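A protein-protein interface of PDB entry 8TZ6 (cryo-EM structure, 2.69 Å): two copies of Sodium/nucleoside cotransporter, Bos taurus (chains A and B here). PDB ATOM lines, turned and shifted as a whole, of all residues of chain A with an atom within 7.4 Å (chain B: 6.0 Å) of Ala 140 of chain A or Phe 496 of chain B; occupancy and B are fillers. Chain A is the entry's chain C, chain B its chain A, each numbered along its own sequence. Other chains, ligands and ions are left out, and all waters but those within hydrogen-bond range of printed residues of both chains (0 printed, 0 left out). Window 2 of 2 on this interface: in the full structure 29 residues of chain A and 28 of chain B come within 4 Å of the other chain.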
ATOM      1  N   TYR A 134       7.414  14.619 -26.160  1.00  0.00           N
ATOM      2  CA  TYR A 134       6.877  13.428 -25.506  1.00  0.00           C
ATOM      3  C   TYR A 134       5.744  12.817 -26.323  1.00  0.00           C
ATOM      4  O   TYR A 134       5.685  11.594 -26.506  1.00  0.00           O
ATOM      5  CB  TYR A 134       6.396  13.777 -24.099  1.00  0.00           C
ATOM      6  CG  TYR A 134       5.683  12.646 -23.393  1.00  0.00           C
ATOM      7  CD1 TYR A 134       6.393  11.610 -22.806  1.00  0.00           C
ATOM      8  CD2 TYR A 134       4.298  12.620 -23.308  1.00  0.00           C
ATOM      9  CE1 TYR A 134       5.745  10.575 -22.159  1.00  0.00           C
ATOM     10  CE2 TYR A 134       3.642  11.592 -22.663  1.00  0.00           C
ATOM     11  CZ  TYR A 134       4.369  10.573 -22.090  1.00  0.00           C
ATOM     12  OH  TYR A 134       3.714   9.550 -21.448  1.00  0.00           O
ATOM     13  N   LEU A 135       4.837  13.656 -26.828  1.00  0.00           N
ATOM     14  CA  LEU A 135       3.732  13.146 -27.631  1.00  0.00           C
ATOM     15  C   LEU A 135       4.238  12.522 -28.926  1.00  0.00           C
ATOM     16  O   LEU A 135       3.685  11.523 -29.400  1.00  0.00           O
ATOM     17  CB  LEU A 135       2.735  14.265 -27.924  1.00  0.00           C
ATOM     18  CG  LEU A 135       2.040  14.862 -26.698  1.00  0.00           C
ATOM     19  CD1 LEU A 135       1.129  16.002 -27.107  1.00  0.00           C
ATOM     20  CD2 LEU A 135       1.260  13.801 -25.942  1.00  0.00           C
ATOM     21  N   ALA A 136       5.282  13.105 -29.517  1.00  0.00           N
ATOM     22  CA  ALA A 136       5.870  12.524 -30.718  1.00  0.00           C
ATOM     23  C   ALA A 136       6.437  11.142 -30.431  1.00  0.00           C
ATOM     24  O   ALA A 136       6.246  10.206 -31.215  1.00  0.00           O
ATOM     25  CB  ALA A 136       6.960  13.444 -31.266  1.00  0.00           C
ATOM     26  N   LEU A 137       7.133  10.994 -29.303  1.00  0.00           N
ATOM     27  CA  LEU A 137       7.640   9.678 -28.928  1.00  0.00           C
ATOM     28  C   LEU A 137       6.498   8.687 -28.764  1.00  0.00           C
ATOM     29  O   LEU A 137       6.562   7.554 -29.259  1.00  0.00           O
ATOM     30  CB  LEU A 137       8.452   9.771 -27.637  1.00  0.00           C
ATOM     31  CG  LEU A 137       9.783  10.518 -27.698  1.00  0.00           C
ATOM     32  CD1 LEU A 137      10.385  10.610 -26.310  1.00  0.00           C
ATOM     33  CD2 LEU A 137      10.747   9.829 -28.647  1.00  0.00           C
ATOM     34  N   VAL A 138       5.432   9.100 -28.075  1.00  0.00           N
ATOM     35  CA  VAL A 138       4.314   8.194 -27.823  1.00  0.00           C
ATOM     36  C   VAL A 138       3.678   7.755 -29.137  1.00  0.00           C
ATOM     37  O   VAL A 138       3.417   6.564 -29.359  1.00  0.00           O
ATOM     38  CB  VAL A 138       3.285   8.860 -26.894  1.00  0.00           C
ATOM     39  CG1 VAL A 138       2.040   8.001 -26.779  1.00  0.00           C
ATOM     40  CG2 VAL A 138       3.889   9.102 -25.525  1.00  0.00           C
ATOM     41  N   ILE A 139       3.417   8.710 -30.031  1.00  0.00           N
ATOM     42  CA  ILE A 139       2.734   8.383 -31.277  1.00  0.00           C
ATOM     43  C   ILE A 139       3.622   7.520 -32.163  1.00  0.00           C
ATOM     44  O   ILE A 139       3.142   6.585 -32.815  1.00  0.00           O
ATOM     45  CB  ILE A 139       2.278   9.665 -32.000  1.00  0.00           C
ATOM     46  CG1 ILE A 139       1.448   9.309 -33.233  1.00  0.00           C
ATOM     47  CG2 ILE A 139       3.469  10.508 -32.401  1.00  0.00           C
ATOM     48  CD1 ILE A 139       0.850  10.507 -33.930  1.00  0.00           C
ATOM     49  N   ALA A 140       4.924   7.811 -32.214  1.00  0.00           N
ATOM     50  CA  ALA A 140       5.826   6.977 -33.000  1.00  0.00           C
ATOM     51  C   ALA A 140       5.869   5.555 -32.457  1.00  0.00           C
ATOM     52  O   ALA A 140       5.853   4.587 -33.228  1.00  0.00           O
ATOM     53  CB  ALA A 140       7.226   7.587 -33.015  1.00  0.00           C
ATOM     54  N   ALA A 141       5.918   5.407 -31.131  1.00  0.00           N
ATOM     55  CA  ALA A 141       5.912   4.075 -30.541  1.00  0.00           C
ATOM     56  C   ALA A 141       4.632   3.329 -30.890  1.00  0.00           C
ATOM     57  O   ALA A 141       4.668   2.138 -31.218  1.00  0.00           O
ATOM     58  CB  ALA A 141       6.079   4.175 -29.025  1.00  0.00           C
ATOM     59  N   CYS A 142       3.489   4.015 -30.827  1.00  0.00           N
ATOM     60  CA  CYS A 142       2.232   3.372 -31.193  1.00  0.00           C
ATOM     61  C   CYS A 142       2.228   2.972 -32.664  1.00  0.00           C
ATOM     62  O   CYS A 142       1.712   1.908 -33.026  1.00  0.00           O
ATOM     63  CB  CYS A 142       1.057   4.300 -30.887  1.00  0.00           C
ATOM     64  SG  CYS A 142       0.745   4.541 -29.124  1.00  0.00           S
ATOM     65  N   VAL A 143       2.797   3.816 -33.526  1.00  0.00           N
ATOM     66  CA  VAL A 143       2.826   3.520 -34.955  1.00  0.00           C
ATOM     67  C   VAL A 143       3.672   2.284 -35.229  1.00  0.00           C
ATOM     68  O   VAL A 143       3.265   1.388 -35.978  1.00  0.00           O
ATOM     69  CB  VAL A 143       3.343   4.739 -35.741  1.00  0.00           C
ATOM     70  CG1 VAL A 143       3.663   4.350 -37.173  1.00  0.00           C
ATOM     71  CG2 VAL A 143       2.321   5.862 -35.712  1.00  0.00           C
ATOM     72  N   MET A 144       4.864   2.216 -34.632  1.00  0.00           N
ATOM     73  CA  MET A 144       5.738   1.074 -34.879  1.00  0.00           C
ATOM     74  C   MET A 144       5.091  -0.224 -34.411  1.00  0.00           C
ATOM     75  O   MET A 144       5.182  -1.253 -35.093  1.00  0.00           O
ATOM     76  CB  MET A 144       7.086   1.283 -34.189  1.00  0.00           C
ATOM     77  CG  MET A 144       7.861   2.478 -34.716  1.00  0.00           C
ATOM     78  SD  MET A 144       9.506   2.640 -33.999  1.00  0.00           S
ATOM     79  CE  MET A 144      10.320   1.204 -34.689  1.00  0.00           C
ATOM     80  N   ASN A 145       4.436  -0.197 -33.253  1.00  0.00           N
ATOM     81  CA  ASN A 145       3.716  -1.357 -32.747  1.00  0.00           C
ATOM     82  C   ASN A 145       2.758  -0.878 -31.668  1.00  0.00           C
ATOM     83  O   ASN A 145       3.165  -0.148 -30.760  1.00  0.00           O
ATOM     84  CB  ASN A 145       4.682  -2.410 -32.192  1.00  0.00           C
ATOM     85  CG  ASN A 145       3.977  -3.684 -31.761  1.00  0.00           C
ATOM     86  OD1 ASN A 145       2.832  -3.656 -31.312  1.00  0.00           O
ATOM     87  ND2 ASN A 145       4.665  -4.812 -31.896  1.00  0.00           N
ATOM     88  N   ARG A 148       2.468  -3.462 -28.238  1.00  0.00           N
ATOM     89  CA  ARG A 148       3.644  -3.302 -27.394  1.00  0.00           C
ATOM     90  C   ARG A 148       3.650  -1.964 -26.664  1.00  0.00           C
ATOM     91  O   ARG A 148       4.208  -1.867 -25.565  1.00  0.00           O
ATOM     92  CB  ARG A 148       4.906  -3.444 -28.244  1.00  0.00           C
ATOM     93  CG  ARG A 148       6.194  -3.489 -27.457  1.00  0.00           C
ATOM     94  CD  ARG A 148       7.357  -3.873 -28.347  1.00  0.00           C
ATOM     95  NE  ARG A 148       7.512  -2.959 -29.470  1.00  0.00           N
ATOM     96  CZ  ARG A 148       8.361  -3.141 -30.471  1.00  0.00           C
ATOM     97  NH1 ARG A 148       9.137  -4.211 -30.534  1.00  0.00           N
ATOM     98  NH2 ARG A 148       8.434  -2.228 -31.435  1.00  0.00           N
ATOM     99  N   ALA A 149       3.045  -0.933 -27.250  1.00  0.00           N
ATOM    100  CA  ALA A 149       3.048   0.412 -26.692  1.00  0.00           C
ATOM    101  C   ALA A 149       1.739   0.775 -26.001  1.00  0.00           C
ATOM    102  O   ALA A 149       1.513   1.952 -25.709  1.00  0.00           O
ATOM    103  CB  ALA A 149       3.349   1.431 -27.789  1.00  0.00           C
ATOM    104  N   LEU A 152       1.862   2.695 -22.351  1.00  0.00           N
ATOM    105  CA  LEU A 152       2.288   4.086 -22.456  1.00  0.00           C
ATOM    106  C   LEU A 152       1.150   4.963 -22.961  1.00  0.00           C
ATOM    107  O   LEU A 152       0.913   6.062 -22.439  1.00  0.00           O
ATOM    108  CB  LEU A 152       3.499   4.176 -23.382  1.00  0.00           C
ATOM    109  CG  LEU A 152       4.120   5.548 -23.626  1.00  0.00           C
ATOM    110  CD1 LEU A 152       4.636   6.150 -22.339  1.00  0.00           C
ATOM    111  CD2 LEU A 152       5.239   5.417 -24.635  1.00  0.00           C
ATOM    112  N   LEU B 492      10.839   1.440 -22.191  1.00  0.00           N
ATOM    113  CA  LEU B 492      10.455   2.443 -23.179  1.00  0.00           C
ATOM    114  C   LEU B 492      11.188   2.231 -24.497  1.00  0.00           C
ATOM    115  O   LEU B 492      10.627   2.477 -25.571  1.00  0.00           O
ATOM    116  CB  LEU B 492      10.731   3.842 -22.630  1.00  0.00           C
ATOM    117  CG  LEU B 492      10.758   4.998 -23.629  1.00  0.00           C
ATOM    118  CD1 LEU B 492       9.431   5.143 -24.336  1.00  0.00           C
ATOM    119  CD2 LEU B 492      11.117   6.284 -22.922  1.00  0.00           C
ATOM    120  N   GLY B 493      12.442   1.783 -24.439  1.00  0.00           N
ATOM    121  CA  GLY B 493      13.225   1.612 -25.648  1.00  0.00           C
ATOM    122  C   GLY B 493      12.804   0.434 -26.498  1.00  0.00           C
ATOM    123  O   GLY B 493      13.108   0.410 -27.694  1.00  0.00           O
ATOM    124  N   ASN B 494      12.117  -0.546 -25.909  1.00  0.00           N
ATOM    125  CA  ASN B 494      11.684  -1.706 -26.677  1.00  0.00           C
ATOM    126  C   ASN B 494      10.593  -1.357 -27.678  1.00  0.00           C
ATOM    127  O   ASN B 494      10.392  -2.103 -28.642  1.00  0.00           O
ATOM    128  CB  ASN B 494      11.193  -2.807 -25.741  1.00  0.00           C
ATOM    129  CG  ASN B 494      11.180  -4.168 -26.401  1.00  0.00           C
ATOM    130  OD1 ASN B 494      11.263  -4.280 -27.623  1.00  0.00           O
ATOM    131  ND2 ASN B 494      11.074  -5.213 -25.595  1.00  0.00           N
ATOM    132  N   MET B 495       9.888  -0.243 -27.477  1.00  0.00           N
ATOM    133  CA  MET B 495       8.861   0.157 -28.432  1.00  0.00           C
ATOM    134  C   MET B 495       9.469   0.393 -29.808  1.00  0.00           C
ATOM    135  O   MET B 495       8.887   0.008 -30.828  1.00  0.00           O
ATOM    136  CB  MET B 495       8.147   1.418 -27.949  1.00  0.00           C
ATOM    137  CG  MET B 495       7.685   1.382 -26.502  1.00  0.00           C
ATOM    138  SD  MET B 495       6.573   0.024 -26.116  1.00  0.00           S
ATOM    139  CE  MET B 495       6.060   0.501 -24.469  1.00  0.00           C
ATOM    140  N   PHE B 496      10.639   1.028 -29.852  1.00  0.00           N
ATOM    141  CA  PHE B 496      11.350   1.299 -31.092  1.00  0.00           C
ATOM    142  C   PHE B 496      12.382   0.227 -31.419  1.00  0.00           C
ATOM    143  O   PHE B 496      13.325   0.494 -32.173  1.00  0.00           O
ATOM    144  CB  PHE B 496      12.027   2.667 -31.013  1.00  0.00           C
ATOM    145  CG  PHE B 496      11.148   3.746 -30.453  1.00  0.00           C
ATOM    146  CD1 PHE B 496      10.327   4.490 -31.279  1.00  0.00           C
ATOM    147  CD2 PHE B 496      11.146   4.016 -29.098  1.00  0.00           C
ATOM    148  CE1 PHE B 496       9.520   5.482 -30.762  1.00  0.00           C
ATOM    149  CE2 PHE B 496      10.341   5.005 -28.577  1.00  0.00           C
ATOM    150  CZ  PHE B 496       9.528   5.739 -29.410  1.00  0.00           C
ATOM    151  N   ASP B 497      12.228  -0.975 -30.865  1.00  0.00           N
ATOM    152  CA  ASP B 497      13.148  -2.084 -31.114  1.00  0.00           C
ATOM    153  C   ASP B 497      14.574  -1.738 -30.701  1.00  0.00           C
ATOM    154  O   ASP B 497      15.540  -2.221 -31.297  1.00  0.00           O
ATOM    155  CB  ASP B 497      13.107  -2.513 -32.583  1.00  0.00           C
ATOM    156  CG  ASP B 497      11.784  -3.143 -32.967  1.00  0.00           C
ATOM    157  OD1 ASP B 497      11.216  -3.883 -32.138  1.00  0.00           O
ATOM    158  OD2 ASP B 497      11.310  -2.896 -34.096  1.00  0.00           O
ATOM    159  N   TYR B 498      14.719  -0.898 -29.677  1.00  0.00           N
ATOM    160  CA  TYR B 498      16.019  -0.525 -29.126  1.00  0.00           C
ATOM    161  C   TYR B 498      15.963  -0.709 -27.615  1.00  0.00           C
ATOM    162  O   TYR B 498      15.819   0.261 -26.861  1.00  0.00           O
ATOM    163  CB  TYR B 498      16.390   0.911 -29.499  1.00  0.00           C
ATOM    164  CG  TYR B 498      17.807   1.289 -29.137  1.00  0.00           C
ATOM    165  CD1 TYR B 498      18.877   0.487 -29.507  1.00  0.00           C
ATOM    166  CD2 TYR B 498      18.078   2.455 -28.437  1.00  0.00           C
ATOM    167  CE1 TYR B 498      20.171   0.827 -29.180  1.00  0.00           C
ATOM    168  CE2 TYR B 498      19.371   2.804 -28.108  1.00  0.00           C
ATOM    169  CZ  TYR B 498      20.413   1.988 -28.483  1.00  0.00           C
ATOM    170  OH  TYR B 498      21.703   2.333 -28.157  1.00  0.00           O
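Among the printed residues, merely in contact across the chains: Met 144 of chain A with Phe 496 of chain B, Leu 137 of chain A with Phe 496 of chain B, Ala 149 of chain A with Met 495 of chain B, Ala 141 of chain A with Met 495 of chain B, Ala 141 of chain A with Phe 496 of chain B and Ala 140 of chain A with Phe 496 of chain B.
Of the 7 printed residues of chain B, 4 touch a printed residue of chain A.
Printed residues of chain B that touch a printed residue of chain A: Asn 494, Met 495, Phe 496 and Asp 497.
Of the 15 printed residues of chain A, 6 touch a printed residue of chain B.
Hydrophobic or aromatic side chains of chain A that line the printed part of chain B: Ala 140, Ala 141, Met 144 and Ala 149.
Among the printed residues, 9 pairs touch across the chains.
The side-chain amide oxygen of Asn 145 of chain A is in hydrogen-bond range of the backbone NH of Arg 148 of chain A.
No position is printed for both chains.
Ala 140 of chain A touches just one residue of chain B: Phe 496.
Of chain A, only Leu 137 (3.5 Å), Ala 140 (3.8 Å), Ala 141 (3.6 Å) and Met 144 (3.4 Å) come within 4 Å of Phe 496 of chain B.
Of the printed residues of chain B, Leu 137 of chain A touches Phe 496 (3.5 Å).
Of the printed residues of chain A, Asn 494 of chain B touches Arg 148.
Printed residues of chain B within 4 Å of Ala 141 of chain A: Met 495 (3.6 Å) and Phe 496 (3.6 Å).
Ala 136 of chain A touches none of the printed residues of chain B.
The nearest residue of chain A that does not touch Phe 496 of chain B is Arg 148 of chain A (4.2 Å).
NH2 of Arg 148 of chain A sits close to O of Met 495 of chain B, 2.4 Å away.
O of Asn 494 of chain B lies close to NH1 of Arg 148 of chain A, 3.1 Å away.
The side-chain carboxylate (OD1) of Asp 497 of chain B is in salt-bridge range of the guanidinium group (NH1) of Arg 148 of chain A (2.6 Å).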
